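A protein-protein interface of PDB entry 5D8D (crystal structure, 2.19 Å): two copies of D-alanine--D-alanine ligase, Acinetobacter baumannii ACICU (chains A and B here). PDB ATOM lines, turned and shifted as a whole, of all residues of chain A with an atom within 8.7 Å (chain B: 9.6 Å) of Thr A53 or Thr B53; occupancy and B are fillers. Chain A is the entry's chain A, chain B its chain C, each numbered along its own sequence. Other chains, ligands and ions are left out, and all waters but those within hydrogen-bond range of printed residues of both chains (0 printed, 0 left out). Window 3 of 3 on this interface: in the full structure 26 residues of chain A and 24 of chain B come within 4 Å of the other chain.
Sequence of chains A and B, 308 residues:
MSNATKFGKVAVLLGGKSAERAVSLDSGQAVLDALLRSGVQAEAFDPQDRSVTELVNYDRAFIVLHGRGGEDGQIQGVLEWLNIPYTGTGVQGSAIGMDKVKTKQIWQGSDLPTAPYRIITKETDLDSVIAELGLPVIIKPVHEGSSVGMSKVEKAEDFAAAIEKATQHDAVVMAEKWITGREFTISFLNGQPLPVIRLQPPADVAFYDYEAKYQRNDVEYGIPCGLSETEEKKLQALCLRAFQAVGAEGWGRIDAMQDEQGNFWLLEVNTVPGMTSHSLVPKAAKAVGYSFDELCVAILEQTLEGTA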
ATOM      1  N   PHE A  45       7.296  12.300  -1.444  1.00  0.00           N
ATOM      2  CA  PHE A  45       7.277  13.752  -1.384  1.00  0.00           C
ATOM      3  C   PHE A  45       8.588  14.124  -0.781  1.00  0.00           C
ATOM      4  O   PHE A  45       8.812  13.873   0.409  1.00  0.00           O
ATOM      5  CB  PHE A  45       6.141  14.222  -0.475  1.00  0.00           C
ATOM      6  CG  PHE A  45       5.829  15.680  -0.586  1.00  0.00           C
ATOM      7  CD1 PHE A  45       6.756  16.645  -0.241  1.00  0.00           C
ATOM      8  CD2 PHE A  45       4.585  16.087  -0.989  1.00  0.00           C
ATOM      9  CE1 PHE A  45       6.463  17.981  -0.336  1.00  0.00           C
ATOM     10  CE2 PHE A  45       4.286  17.420  -1.083  1.00  0.00           C
ATOM     11  CZ  PHE A  45       5.220  18.368  -0.747  1.00  0.00           C
ATOM     12  N   PRO A  47      10.725  17.104   0.325  1.00  0.00           N
ATOM     13  CA  PRO A  47      10.583  18.548   0.554  1.00  0.00           C
ATOM     14  C   PRO A  47      11.778  19.386   0.171  1.00  0.00           C
ATOM     15  O   PRO A  47      11.667  20.612   0.167  1.00  0.00           O
ATOM     16  CB  PRO A  47      10.282  18.650   2.045  1.00  0.00           C
ATOM     17  CG  PRO A  47      10.909  17.435   2.622  1.00  0.00           C
ATOM     18  CD  PRO A  47      10.763  16.358   1.593  1.00  0.00           C
ATOM     19  N   ARG A  50      10.185  19.640  -3.720  1.00  0.00           N
ATOM     20  CA  ARG A  50       8.774  20.065  -3.793  1.00  0.00           C
ATOM     21  C   ARG A  50       8.481  20.947  -2.611  1.00  0.00           C
ATOM     22  O   ARG A  50       8.709  20.525  -1.463  1.00  0.00           O
ATOM     23  CB  ARG A  50       7.827  18.847  -3.651  1.00  0.00           C
ATOM     24  CG  ARG A  50       7.068  18.437  -4.887  1.00  0.00           C
ATOM     25  CD  ARG A  50       5.545  18.546  -4.786  1.00  0.00           C
ATOM     26  NE  ARG A  50       4.942  17.238  -4.574  1.00  0.00           N
ATOM     27  CZ  ARG A  50       3.659  16.938  -4.770  1.00  0.00           C
ATOM     28  NH1 ARG A  50       2.770  17.845  -5.162  1.00  0.00           N
ATOM     29  NH2 ARG A  50       3.248  15.693  -4.549  1.00  0.00           N
ATOM     30  N   SER A  51       7.915  22.129  -2.878  1.00  0.00           N
ATOM     31  CA  SER A  51       7.490  23.021  -1.827  1.00  0.00           C
ATOM     32  C   SER A  51       6.626  22.269  -0.846  1.00  0.00           C
ATOM     33  O   SER A  51       5.699  21.615  -1.259  1.00  0.00           O
ATOM     34  CB  SER A  51       6.690  24.165  -2.392  1.00  0.00           C
ATOM     35  OG  SER A  51       6.322  25.062  -1.367  1.00  0.00           O
ATOM     36  N   VAL A  52       6.927  22.373   0.449  1.00  0.00           N
ATOM     37  CA  VAL A  52       6.021  21.847   1.504  1.00  0.00           C
ATOM     38  C   VAL A  52       4.568  22.355   1.488  1.00  0.00           C
ATOM     39  O   VAL A  52       3.688  21.718   2.034  1.00  0.00           O
ATOM     40  CB  VAL A  52       6.557  22.089   2.913  1.00  0.00           C
ATOM     41  CG1 VAL A  52       7.913  21.432   3.064  1.00  0.00           C
ATOM     42  CG2 VAL A  52       6.648  23.572   3.238  1.00  0.00           C
ATOM     43  N   THR A  53       4.302  23.482   0.851  1.00  0.00           N
ATOM     44  CA  THR A  53       2.902  23.932   0.648  1.00  0.00           C
ATOM     45  C   THR A  53       2.053  22.981  -0.158  1.00  0.00           C
ATOM     46  O   THR A  53       0.851  22.955   0.001  1.00  0.00           O
ATOM     47  CB  THR A  53       2.816  25.331   0.001  1.00  0.00           C
ATOM     48  OG1 THR A  53       3.463  25.337  -1.287  1.00  0.00           O
ATOM     49  CG2 THR A  53       3.457  26.352   0.950  1.00  0.00           C
ATOM     50  N   GLU A  54       2.699  22.175  -0.990  1.00  0.00           N
ATOM     51  CA  GLU A  54       2.021  21.159  -1.833  1.00  0.00           C
ATOM     52  C   GLU A  54       1.538  19.897  -1.090  1.00  0.00           C
ATOM     53  O   GLU A  54       0.870  19.036  -1.671  1.00  0.00           O
ATOM     54  CB  GLU A  54       2.923  20.805  -3.013  1.00  0.00           C
ATOM     55  CG  GLU A  54       3.274  22.035  -3.857  1.00  0.00           C
ATOM     56  CD  GLU A  54       4.110  21.732  -5.095  1.00  0.00           C
ATOM     57  OE1 GLU A  54       3.851  20.698  -5.745  1.00  0.00           O
ATOM     58  OE2 GLU A  54       5.007  22.537  -5.430  1.00  0.00           O
ATOM     59  N   LEU A  55       1.834  19.832   0.206  1.00  0.00           N
ATOM     60  CA  LEU A  55       1.306  18.826   1.103  1.00  0.00           C
ATOM     61  C   LEU A  55      -0.182  18.937   1.278  1.00  0.00           C
ATOM     62  O   LEU A  55      -0.830  17.987   1.722  1.00  0.00           O
ATOM     63  CB  LEU A  55       1.988  18.910   2.494  1.00  0.00           C
ATOM     64  CG  LEU A  55       3.404  18.305   2.583  1.00  0.00           C
ATOM     65  CD1 LEU A  55       4.117  18.724   3.859  1.00  0.00           C
ATOM     66  CD2 LEU A  55       3.361  16.790   2.516  1.00  0.00           C
ATOM     67  N   VAL A  56      -0.736  20.088   0.928  1.00  0.00           N
ATOM     68  CA  VAL A  56      -2.184  20.287   1.008  1.00  0.00           C
ATOM     69  C   VAL A  56      -2.955  19.323   0.087  1.00  0.00           C
ATOM     70  O   VAL A  56      -4.098  18.980   0.365  1.00  0.00           O
ATOM     71  CB  VAL A  56      -2.518  21.781   0.748  1.00  0.00           C
ATOM     72  CG1 VAL A  56      -2.529  22.100  -0.751  1.00  0.00           C
ATOM     73  CG2 VAL A  56      -3.820  22.164   1.428  1.00  0.00           C
ATOM     74  N   ASN A  57      -2.293  18.822  -0.964  1.00  0.00           N
ATOM     75  CA  ASN A  57      -2.846  17.772  -1.849  1.00  0.00           C
ATOM     76  C   ASN A  57      -2.977  16.347  -1.236  1.00  0.00           C
ATOM     77  O   ASN A  57      -3.310  15.418  -1.951  1.00  0.00           O
ATOM     78  CB  ASN A  57      -1.984  17.689  -3.111  1.00  0.00           C
ATOM     79  CG  ASN A  57      -1.964  18.987  -3.906  1.00  0.00           C
ATOM     80  OD1 ASN A  57      -2.996  19.461  -4.359  1.00  0.00           O
ATOM     81  ND2 ASN A  57      -0.787  19.580  -4.051  1.00  0.00           N
ATOM     82  N   TYR A  58      -2.733  16.179   0.071  1.00  0.00           N
ATOM     83  CA  TYR A  58      -2.731  14.874   0.714  1.00  0.00           C
ATOM     84  C   TYR A  58      -3.606  14.836   1.961  1.00  0.00           C
ATOM     85  O   TYR A  58      -3.793  15.829   2.645  1.00  0.00           O
ATOM     86  CB  TYR A  58      -1.286  14.457   1.070  1.00  0.00           C
ATOM     87  CG  TYR A  58      -0.438  14.289  -0.156  1.00  0.00           C
ATOM     88  CD1 TYR A  58      -0.447  13.105  -0.883  1.00  0.00           C
ATOM     89  CD2 TYR A  58       0.311  15.336  -0.631  1.00  0.00           C
ATOM     90  CE1 TYR A  58       0.313  12.959  -2.039  1.00  0.00           C
ATOM     91  CE2 TYR A  58       1.057  15.219  -1.795  1.00  0.00           C
ATOM     92  CZ  TYR A  58       1.057  14.035  -2.494  1.00  0.00           C
ATOM     93  OH  TYR A  58       1.832  13.966  -3.616  1.00  0.00           O
ATOM     94  N   ILE A  75       9.209  19.994  10.136  1.00  0.00           N
ATOM     95  CA  ILE A  75       8.243  19.458   9.196  1.00  0.00           C
ATOM     96  C   ILE A  75       6.923  19.224   9.931  1.00  0.00           C
ATOM     97  O   ILE A  75       5.870  19.353   9.320  1.00  0.00           O
ATOM     98  CB  ILE A  75       8.745  18.185   8.459  1.00  0.00           C
ATOM     99  CG1 ILE A  75       7.849  17.804   7.254  1.00  0.00           C
ATOM    100  CG2 ILE A  75       8.791  16.987   9.412  1.00  0.00           C
ATOM    101  CD1 ILE A  75       7.837  18.777   6.099  1.00  0.00           C
ATOM    102  N   VAL A  78       4.983  22.472   9.918  1.00  0.00           N
ATOM    103  CA  VAL A  78       4.205  22.731   8.682  1.00  0.00           C
ATOM    104  C   VAL A  78       2.955  21.872   8.618  1.00  0.00           C
ATOM    105  O   VAL A  78       1.889  22.333   8.195  1.00  0.00           O
ATOM    106  CB  VAL A  78       4.987  22.768   7.305  1.00  0.00           C
ATOM    107  CG1 VAL A  78       6.495  22.987   7.442  1.00  0.00           C
ATOM    108  CG2 VAL A  78       4.657  21.610   6.406  1.00  0.00           C
ATOM    109  N   TRP A  81       0.328  23.373  10.871  1.00  0.00           N
ATOM    110  CA  TRP A  81      -0.144  24.586  10.207  1.00  0.00           C
ATOM    111  C   TRP A  81      -1.147  24.289   9.095  1.00  0.00           C
ATOM    112  O   TRP A  81      -2.209  24.888   9.034  1.00  0.00           O
ATOM    113  CB  TRP A  81       1.056  25.359   9.638  1.00  0.00           C
ATOM    114  CG  TRP A  81       0.720  26.706   9.212  1.00  0.00           C
ATOM    115  CD1 TRP A  81       0.551  27.130   7.936  1.00  0.00           C
ATOM    116  CD2 TRP A  81       0.471  27.842  10.050  1.00  0.00           C
ATOM    117  NE1 TRP A  81       0.229  28.460   7.911  1.00  0.00           N
ATOM    118  CE2 TRP A  81       0.153  28.921   9.198  1.00  0.00           C
ATOM    119  CE3 TRP A  81       0.455  28.045  11.430  1.00  0.00           C
ATOM    120  CZ2 TRP A  81      -0.167  30.203   9.690  1.00  0.00           C
ATOM    121  CZ3 TRP A  81       0.122  29.299  11.914  1.00  0.00           C
ATOM    122  CH2 TRP A  81      -0.170  30.365  11.046  1.00  0.00           C
ATOM    123  N   LEU A  82      -0.825  23.315   8.243  1.00  0.00           N
ATOM    124  CA  LEU A  82      -1.748  22.822   7.183  1.00  0.00           C
ATOM    125  C   LEU A  82      -2.940  21.922   7.676  1.00  0.00           C
ATOM    126  O   LEU A  82      -3.798  21.543   6.911  1.00  0.00           O
ATOM    127  CB  LEU A  82      -0.892  22.057   6.171  1.00  0.00           C
ATOM    128  CG  LEU A  82      -0.194  22.773   5.017  1.00  0.00           C
ATOM    129  CD1 LEU A  82      -0.316  24.274   4.953  1.00  0.00           C
ATOM    130  CD2 LEU A  82       1.250  22.405   4.989  1.00  0.00           C
ATOM    131  N   ILE A  84      -2.811  18.699   8.657  1.00  0.00           N
ATOM    132  CA  ILE A  84      -2.678  17.373   8.049  1.00  0.00           C
ATOM    133  C   ILE A  84      -2.140  16.447   9.119  1.00  0.00           C
ATOM    134  O   ILE A  84      -1.065  16.702   9.658  1.00  0.00           O
ATOM    135  CB  ILE A  84      -1.719  17.433   6.860  1.00  0.00           C
ATOM    136  CG1 ILE A  84      -2.299  18.357   5.796  1.00  0.00           C
ATOM    137  CG2 ILE A  84      -1.464  16.053   6.277  1.00  0.00           C
ATOM    138  CD1 ILE A  84      -1.315  18.683   4.738  1.00  0.00           C
ATOM    139  N   PHE B  45       0.299  40.488   6.986  1.00  0.00           N
ATOM    140  CA  PHE B  45       0.074  39.135   6.524  1.00  0.00           C
ATOM    141  C   PHE B  45      -0.683  38.389   7.617  1.00  0.00           C
ATOM    142  O   PHE B  45      -0.110  37.898   8.615  1.00  0.00           O
ATOM    143  CB  PHE B  45       1.418  38.462   6.172  1.00  0.00           C
ATOM    144  CG  PHE B  45       1.283  37.206   5.324  1.00  0.00           C
ATOM    145  CD1 PHE B  45       0.681  36.058   5.826  1.00  0.00           C
ATOM    146  CD2 PHE B  45       1.762  37.174   4.027  1.00  0.00           C
ATOM    147  CE1 PHE B  45       0.559  34.913   5.059  1.00  0.00           C
ATOM    148  CE2 PHE B  45       1.636  36.025   3.254  1.00  0.00           C
ATOM    149  CZ  PHE B  45       1.029  34.888   3.783  1.00  0.00           C
ATOM    150  N   PRO B  47      -2.864  35.214   8.338  1.00  0.00           N
ATOM    151  CA  PRO B  47      -3.202  33.899   7.803  1.00  0.00           C
ATOM    152  C   PRO B  47      -4.677  33.603   7.559  1.00  0.00           C
ATOM    153  O   PRO B  47      -4.982  32.700   6.807  1.00  0.00           O
ATOM    154  CB  PRO B  47      -2.662  32.951   8.875  1.00  0.00           C
ATOM    155  CG  PRO B  47      -1.552  33.687   9.505  1.00  0.00           C
ATOM    156  CD  PRO B  47      -2.043  35.095   9.558  1.00  0.00           C
ATOM    157  N   ARG B  50      -5.029  35.083   4.066  1.00  0.00           N
ATOM    158  CA  ARG B  50      -3.958  34.797   3.113  1.00  0.00           C
ATOM    159  C   ARG B  50      -3.743  33.293   2.955  1.00  0.00           C
ATOM    160  O   ARG B  50      -4.159  32.483   3.809  1.00  0.00           O
ATOM    161  CB  ARG B  50      -2.671  35.432   3.606  1.00  0.00           C
ATOM    162  CG  ARG B  50      -2.658  36.946   3.557  1.00  0.00           C
ATOM    163  CD  ARG B  50      -2.098  37.493   2.262  1.00  0.00           C
ATOM    164  NE  ARG B  50      -1.299  38.682   2.485  1.00  0.00           N
ATOM    165  CZ  ARG B  50      -0.271  39.085   1.718  1.00  0.00           C
ATOM    166  NH1 ARG B  50       0.132  38.428   0.629  1.00  0.00           N
ATOM    167  NH2 ARG B  50       0.392  40.187   2.051  1.00  0.00           N
ATOM    168  N   SER B  51      -3.104  32.947   1.842  1.00  0.00           N
ATOM    169  CA  SER B  51      -2.594  31.600   1.557  1.00  0.00           C
ATOM    170  C   SER B  51      -1.131  31.527   1.962  1.00  0.00           C
ATOM    171  O   SER B  51      -0.377  32.449   1.652  1.00  0.00           O
ATOM    172  CB  SER B  51      -2.725  31.293   0.032  1.00  0.00           C
ATOM    173  OG  SER B  51      -1.966  30.159  -0.418  1.00  0.00           O
ATOM    174  N   VAL B  52      -0.733  30.417   2.606  1.00  0.00           N
ATOM    175  CA  VAL B  52       0.689  30.072   2.841  1.00  0.00           C
ATOM    176  C   VAL B  52       1.633  30.254   1.653  1.00  0.00           C
ATOM    177  O   VAL B  52       2.784  30.616   1.839  1.00  0.00           O
ATOM    178  CB  VAL B  52       0.917  28.591   3.241  1.00  0.00           C
ATOM    179  CG1 VAL B  52       0.431  28.340   4.636  1.00  0.00           C
ATOM    180  CG2 VAL B  52       0.287  27.606   2.241  1.00  0.00           C
ATOM    181  N   THR B  53       1.143  29.976   0.459  1.00  0.00           N
ATOM    182  CA  THR B  53       1.941  30.088  -0.749  1.00  0.00           C
ATOM    183  C   THR B  53       2.383  31.496  -0.955  1.00  0.00           C
ATOM    184  O   THR B  53       3.305  31.725  -1.730  1.00  0.00           O
ATOM    185  CB  THR B  53       1.198  29.624  -2.031  1.00  0.00           C
ATOM    186  OG1 THR B  53       0.000  30.395  -2.263  1.00  0.00           O
ATOM    187  CG2 THR B  53       0.812  28.168  -1.910  1.00  0.00           C
ATOM    188  N   GLU B  54       1.764  32.456  -0.256  1.00  0.00           N
ATOM    189  CA  GLU B  54       2.155  33.861  -0.451  1.00  0.00           C
ATOM    190  C   GLU B  54       3.368  34.287   0.359  1.00  0.00           C
ATOM    191  O   GLU B  54       3.947  35.330   0.050  1.00  0.00           O
ATOM    192  CB  GLU B  54       0.984  34.794  -0.176  1.00  0.00           C
ATOM    193  CG  GLU B  54      -0.221  34.530  -1.046  1.00  0.00           C
ATOM    194  CD  GLU B  54      -1.288  35.579  -0.835  1.00  0.00           C
ATOM    195  OE1 GLU B  54      -1.004  36.724  -1.228  1.00  0.00           O
ATOM    196  OE2 GLU B  54      -2.371  35.282  -0.253  1.00  0.00           O
ATOM    197  N   LEU B  55       3.763  33.497   1.366  1.00  0.00           N
ATOM    198  CA  LEU B  55       4.941  33.816   2.199  1.00  0.00           C
ATOM    199  C   LEU B  55       6.200  33.927   1.386  1.00  0.00           C
ATOM    200  O   LEU B  55       7.109  34.657   1.752  1.00  0.00           O
ATOM    201  CB  LEU B  55       5.160  32.780   3.321  1.00  0.00           C
ATOM    202  CG  LEU B  55       4.119  32.710   4.450  1.00  0.00           C
ATOM    203  CD1 LEU B  55       4.260  31.465   5.345  1.00  0.00           C
ATOM    204  CD2 LEU B  55       4.150  33.987   5.279  1.00  0.00           C
ATOM    205  N   VAL B  56       6.249  33.197   0.280  1.00  0.00           N
ATOM    206  CA  VAL B  56       7.424  33.183  -0.604  1.00  0.00           C
ATOM    207  C   VAL B  56       7.656  34.528  -1.338  1.00  0.00           C
ATOM    208  O   VAL B  56       8.762  34.815  -1.776  1.00  0.00           O
ATOM    209  CB  VAL B  56       7.331  31.982  -1.588  1.00  0.00           C
ATOM    210  CG1 VAL B  56       6.281  32.230  -2.670  1.00  0.00           C
ATOM    211  CG2 VAL B  56       8.695  31.682  -2.197  1.00  0.00           C
ATOM    212  N   ASN B  57       6.633  35.369  -1.419  1.00  0.00           N
ATOM    213  CA  ASN B  57       6.812  36.767  -1.868  1.00  0.00           C
ATOM    214  C   ASN B  57       7.587  37.717  -0.942  1.00  0.00           C
ATOM    215  O   ASN B  57       7.866  38.833  -1.356  1.00  0.00           O
ATOM    216  CB  ASN B  57       5.459  37.406  -2.100  1.00  0.00           C
ATOM    217  CG  ASN B  57       4.617  36.635  -3.088  1.00  0.00           C
ATOM    218  OD1 ASN B  57       5.097  36.262  -4.127  1.00  0.00           O
ATOM    219  ND2 ASN B  57       3.369  36.386  -2.757  1.00  0.00           N
ATOM    220  N   TYR B  58       7.944  37.302   0.279  1.00  0.00           N
ATOM    221  CA  TYR B  58       8.644  38.169   1.213  1.00  0.00           C
ATOM    222  C   TYR B  58      10.046  37.699   1.474  1.00  0.00           C
ATOM    223  O   TYR B  58      10.280  36.540   1.467  1.00  0.00           O
ATOM    224  CB  TYR B  58       7.832  38.242   2.536  1.00  0.00           C
ATOM    225  CG  TYR B  58       6.459  38.813   2.271  1.00  0.00           C
ATOM    226  CD1 TYR B  58       6.267  40.186   2.215  1.00  0.00           C
ATOM    227  CD2 TYR B  58       5.380  37.986   1.973  1.00  0.00           C
ATOM    228  CE1 TYR B  58       5.019  40.729   1.921  1.00  0.00           C
ATOM    229  CE2 TYR B  58       4.130  38.520   1.660  1.00  0.00           C
ATOM    230  CZ  TYR B  58       3.958  39.889   1.632  1.00  0.00           C
ATOM    231  OH  TYR B  58       2.733  40.430   1.356  1.00  0.00           O
ATOM    232  N   ILE B  75       4.289  28.111  12.784  1.00  0.00           N
ATOM    233  CA  ILE B  75       4.657  29.066  11.751  1.00  0.00           C
ATOM    234  C   ILE B  75       6.159  29.098  11.573  1.00  0.00           C
ATOM    235  O   ILE B  75       6.635  29.271  10.448  1.00  0.00           O
ATOM    236  CB  ILE B  75       4.106  30.488  12.022  1.00  0.00           C
ATOM    237  CG1 ILE B  75       4.153  31.342  10.746  1.00  0.00           C
ATOM    238  CG2 ILE B  75       4.852  31.207  13.158  1.00  0.00           C
ATOM    239  CD1 ILE B  75       3.345  30.809   9.582  1.00  0.00           C
ATOM    240  N   GLY B  77       8.220  26.597  11.931  1.00  0.00           N
ATOM    241  CA  GLY B  77       8.455  25.446  11.101  1.00  0.00           C
ATOM    242  C   GLY B  77       8.232  25.728   9.614  1.00  0.00           C
ATOM    243  O   GLY B  77       9.102  25.428   8.803  1.00  0.00           O
ATOM    244  N   VAL B  78       7.103  26.352   9.267  1.00  0.00           N
ATOM    245  CA  VAL B  78       6.817  26.593   7.857  1.00  0.00           C
ATOM    246  C   VAL B  78       7.837  27.537   7.244  1.00  0.00           C
ATOM    247  O   VAL B  78       8.288  27.306   6.127  1.00  0.00           O
ATOM    248  CB  VAL B  78       5.350  26.975   7.514  1.00  0.00           C
ATOM    249  CG1 VAL B  78       4.389  26.742   8.654  1.00  0.00           C
ATOM    250  CG2 VAL B  78       5.243  28.369   6.931  1.00  0.00           C
ATOM    251  N   LEU B  79       8.236  28.548   7.992  1.00  0.00           N
ATOM    252  CA  LEU B  79       9.258  29.517   7.528  1.00  0.00           C
ATOM    253  C   LEU B  79      10.654  28.923   7.424  1.00  0.00           C
ATOM    254  O   LEU B  79      11.415  29.297   6.535  1.00  0.00           O
ATOM    255  CB  LEU B  79       9.287  30.764   8.440  1.00  0.00           C
ATOM    256  CG  LEU B  79       7.998  31.611   8.441  1.00  0.00           C
ATOM    257  CD1 LEU B  79       7.850  32.443   9.702  1.00  0.00           C
ATOM    258  CD2 LEU B  79       8.000  32.532   7.232  1.00  0.00           C
ATOM    259  N   TRP B  81      11.278  25.819   6.544  1.00  0.00           N
ATOM    260  CA  TRP B  81      11.203  25.062   5.303  1.00  0.00           C
ATOM    261  C   TRP B  81      11.088  25.892   4.052  1.00  0.00           C
ATOM    262  O   TRP B  81      11.500  25.457   3.002  1.00  0.00           O
ATOM    263  CB  TRP B  81      10.045  24.041   5.340  1.00  0.00           C
ATOM    264  CG  TRP B  81      10.504  22.737   5.911  1.00  0.00           C
ATOM    265  CD1 TRP B  81      10.176  22.207   7.127  1.00  0.00           C
ATOM    266  CD2 TRP B  81      11.427  21.831   5.306  1.00  0.00           C
ATOM    267  NE1 TRP B  81      10.806  21.007   7.295  1.00  0.00           N
ATOM    268  CE2 TRP B  81      11.581  20.746   6.190  1.00  0.00           C
ATOM    269  CE3 TRP B  81      12.092  21.802   4.084  1.00  0.00           C
ATOM    270  CZ2 TRP B  81      12.406  19.631   5.888  1.00  0.00           C
ATOM    271  CZ3 TRP B  81      12.922  20.722   3.794  1.00  0.00           C
ATOM    272  CH2 TRP B  81      13.065  19.646   4.696  1.00  0.00           C
ATOM    273  N   LEU B  82      10.492  27.056   4.151  1.00  0.00           N
ATOM    274  CA  LEU B  82      10.463  27.994   3.018  1.00  0.00           C
ATOM    275  C   LEU B  82      11.729  28.833   2.938  1.00  0.00           C
ATOM    276  O   LEU B  82      11.836  29.647   2.031  1.00  0.00           O
ATOM    277  CB  LEU B  82       9.239  28.894   3.108  1.00  0.00           C
ATOM    278  CG  LEU B  82       7.946  28.503   2.380  1.00  0.00           C
ATOM    279  CD1 LEU B  82       7.782  27.068   1.976  1.00  0.00           C
ATOM    280  CD2 LEU B  82       6.723  28.969   3.152  1.00  0.00           C
ATOM    281  N   ILE B  84      12.656  31.349   4.906  1.00  0.00           N
ATOM    282  CA  ILE B  84      12.328  32.721   5.144  1.00  0.00           C
ATOM    283  C   ILE B  84      12.882  33.074   6.531  1.00  0.00           C
ATOM    284  O   ILE B  84      12.439  32.532   7.527  1.00  0.00           O
ATOM    285  CB  ILE B  84      10.802  32.960   5.002  1.00  0.00           C
ATOM    286  CG1 ILE B  84      10.367  32.704   3.559  1.00  0.00           C
ATOM    287  CG2 ILE B  84      10.426  34.408   5.386  1.00  0.00           C
ATOM    288  CD1 ILE B  84       8.859  32.726   3.345  1.00  0.00           C
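N of Ile A75 sits close to NE1 of Trp B81, 3.4 Å away.
OG of Ser A51 lies within hydrogen-bond range of OG1 of Thr A53.
OG of Ser B51 lies within hydrogen-bond range of OG1 of Thr B53, at 2.7 Å.
Among the printed residues, merely in contact across the chains: Pro A47 with Trp B81 (3.7 Å), Val A52 with Leu B82 (3.9 Å), Thr A53 with Val B52 (3.6 Å), Thr A53 with Thr B53 (3.9 Å), Val A78 with Gly B77 (3.8 Å), Val A78 with Val B78 (3.6 Å), Val A78 with Trp B81 (3.8 Å), Trp A81 with Pro B47 (3.8 Å), Trp A81 with Val B52 (3.3 Å), Trp A81 with Ile B75 (3.6 Å) and Trp A81 with Val B78 (3.7 Å).
Thr A53 touches just these residues of chain B: Val B52 and Thr B53.
Thr B53 touches just one residue of chain A: Thr A53 (3.9 Å).
Val A52 touches just one residue of chain B: Leu B82 (3.9 Å).
Of the printed residues of chain A, Val B52 touches Thr A53 (3.6 Å) and Trp A81 (3.3 Å).
Printed residues of chain A within 4 Å of Ile B75: Trp A81.
Of the printed residues of chain A, Gly B77 touches Val A78.
Printed residues of chain A within 4 Å of Leu B82: Val A52 (3.9 Å).
Printed residues of chain A within 4 Å of Trp B81: Pro A47 (3.7 Å), Ile A75 (3.4 Å) and Val A78 (3.8 Å).
Of the printed residues of chain B, Val A78 touches Gly B77 (3.8 Å), Val B78 (3.6 Å) and Trp B81 (3.8 Å).
Glu A54 touches none of the printed residues of chain B.
Leu A55 touches none of the printed residues of chain B.
The nearest printed residue of chain A that does not touch Thr B53 is Ser A51 (6.3 Å).
Printed residues of chain B that touch a printed residue of chain A: Pro B47, Val B52, Thr B53, Ile B75, Gly B77, Val B78, Trp B81 and Leu B82.
Hydrophobic or aromatic side chains of chain B that line the printed part of chain A: Pro B47, Val B52, Ile B75, Val B78, Trp B81 and Leu B82.
Of the 16 printed residues of chain A, 6 touch a printed residue of chain B.
Printed residues of chain A that touch a printed residue of chain B: Pro A47, Val A52, Thr A53, Ile A75, Val A78 and Trp A81.
Among the printed residues, no Asp or Glu carboxylate lies within 4 Å of a Lys or Arg side-chain nitrogen of the other chain.
Pro A47 touches Trp B81, and with the chains exchanged Trp A81 touches Pro B47.
Thr A53 touches Val B52, but with the chains exchanged Val A52 does not touch Thr B53 (7.7 Å).
Ile A75 touches Trp B81, and with the chains exchanged Trp A81 touches Ile B75.
Trp A81 touches Val B52, but with the chains exchanged Val A52 does not touch Trp B81 (4.02 Å).
Positions printed for both chains: 45, 47, 50, 51, 52, 53, 54, 55, 56, 57, 58, 75, 78, 81, 82 and 84.
Of the 12 pairs that touch across the chains among the printed residues, 8 have their exchanged pair printed and touching as well.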
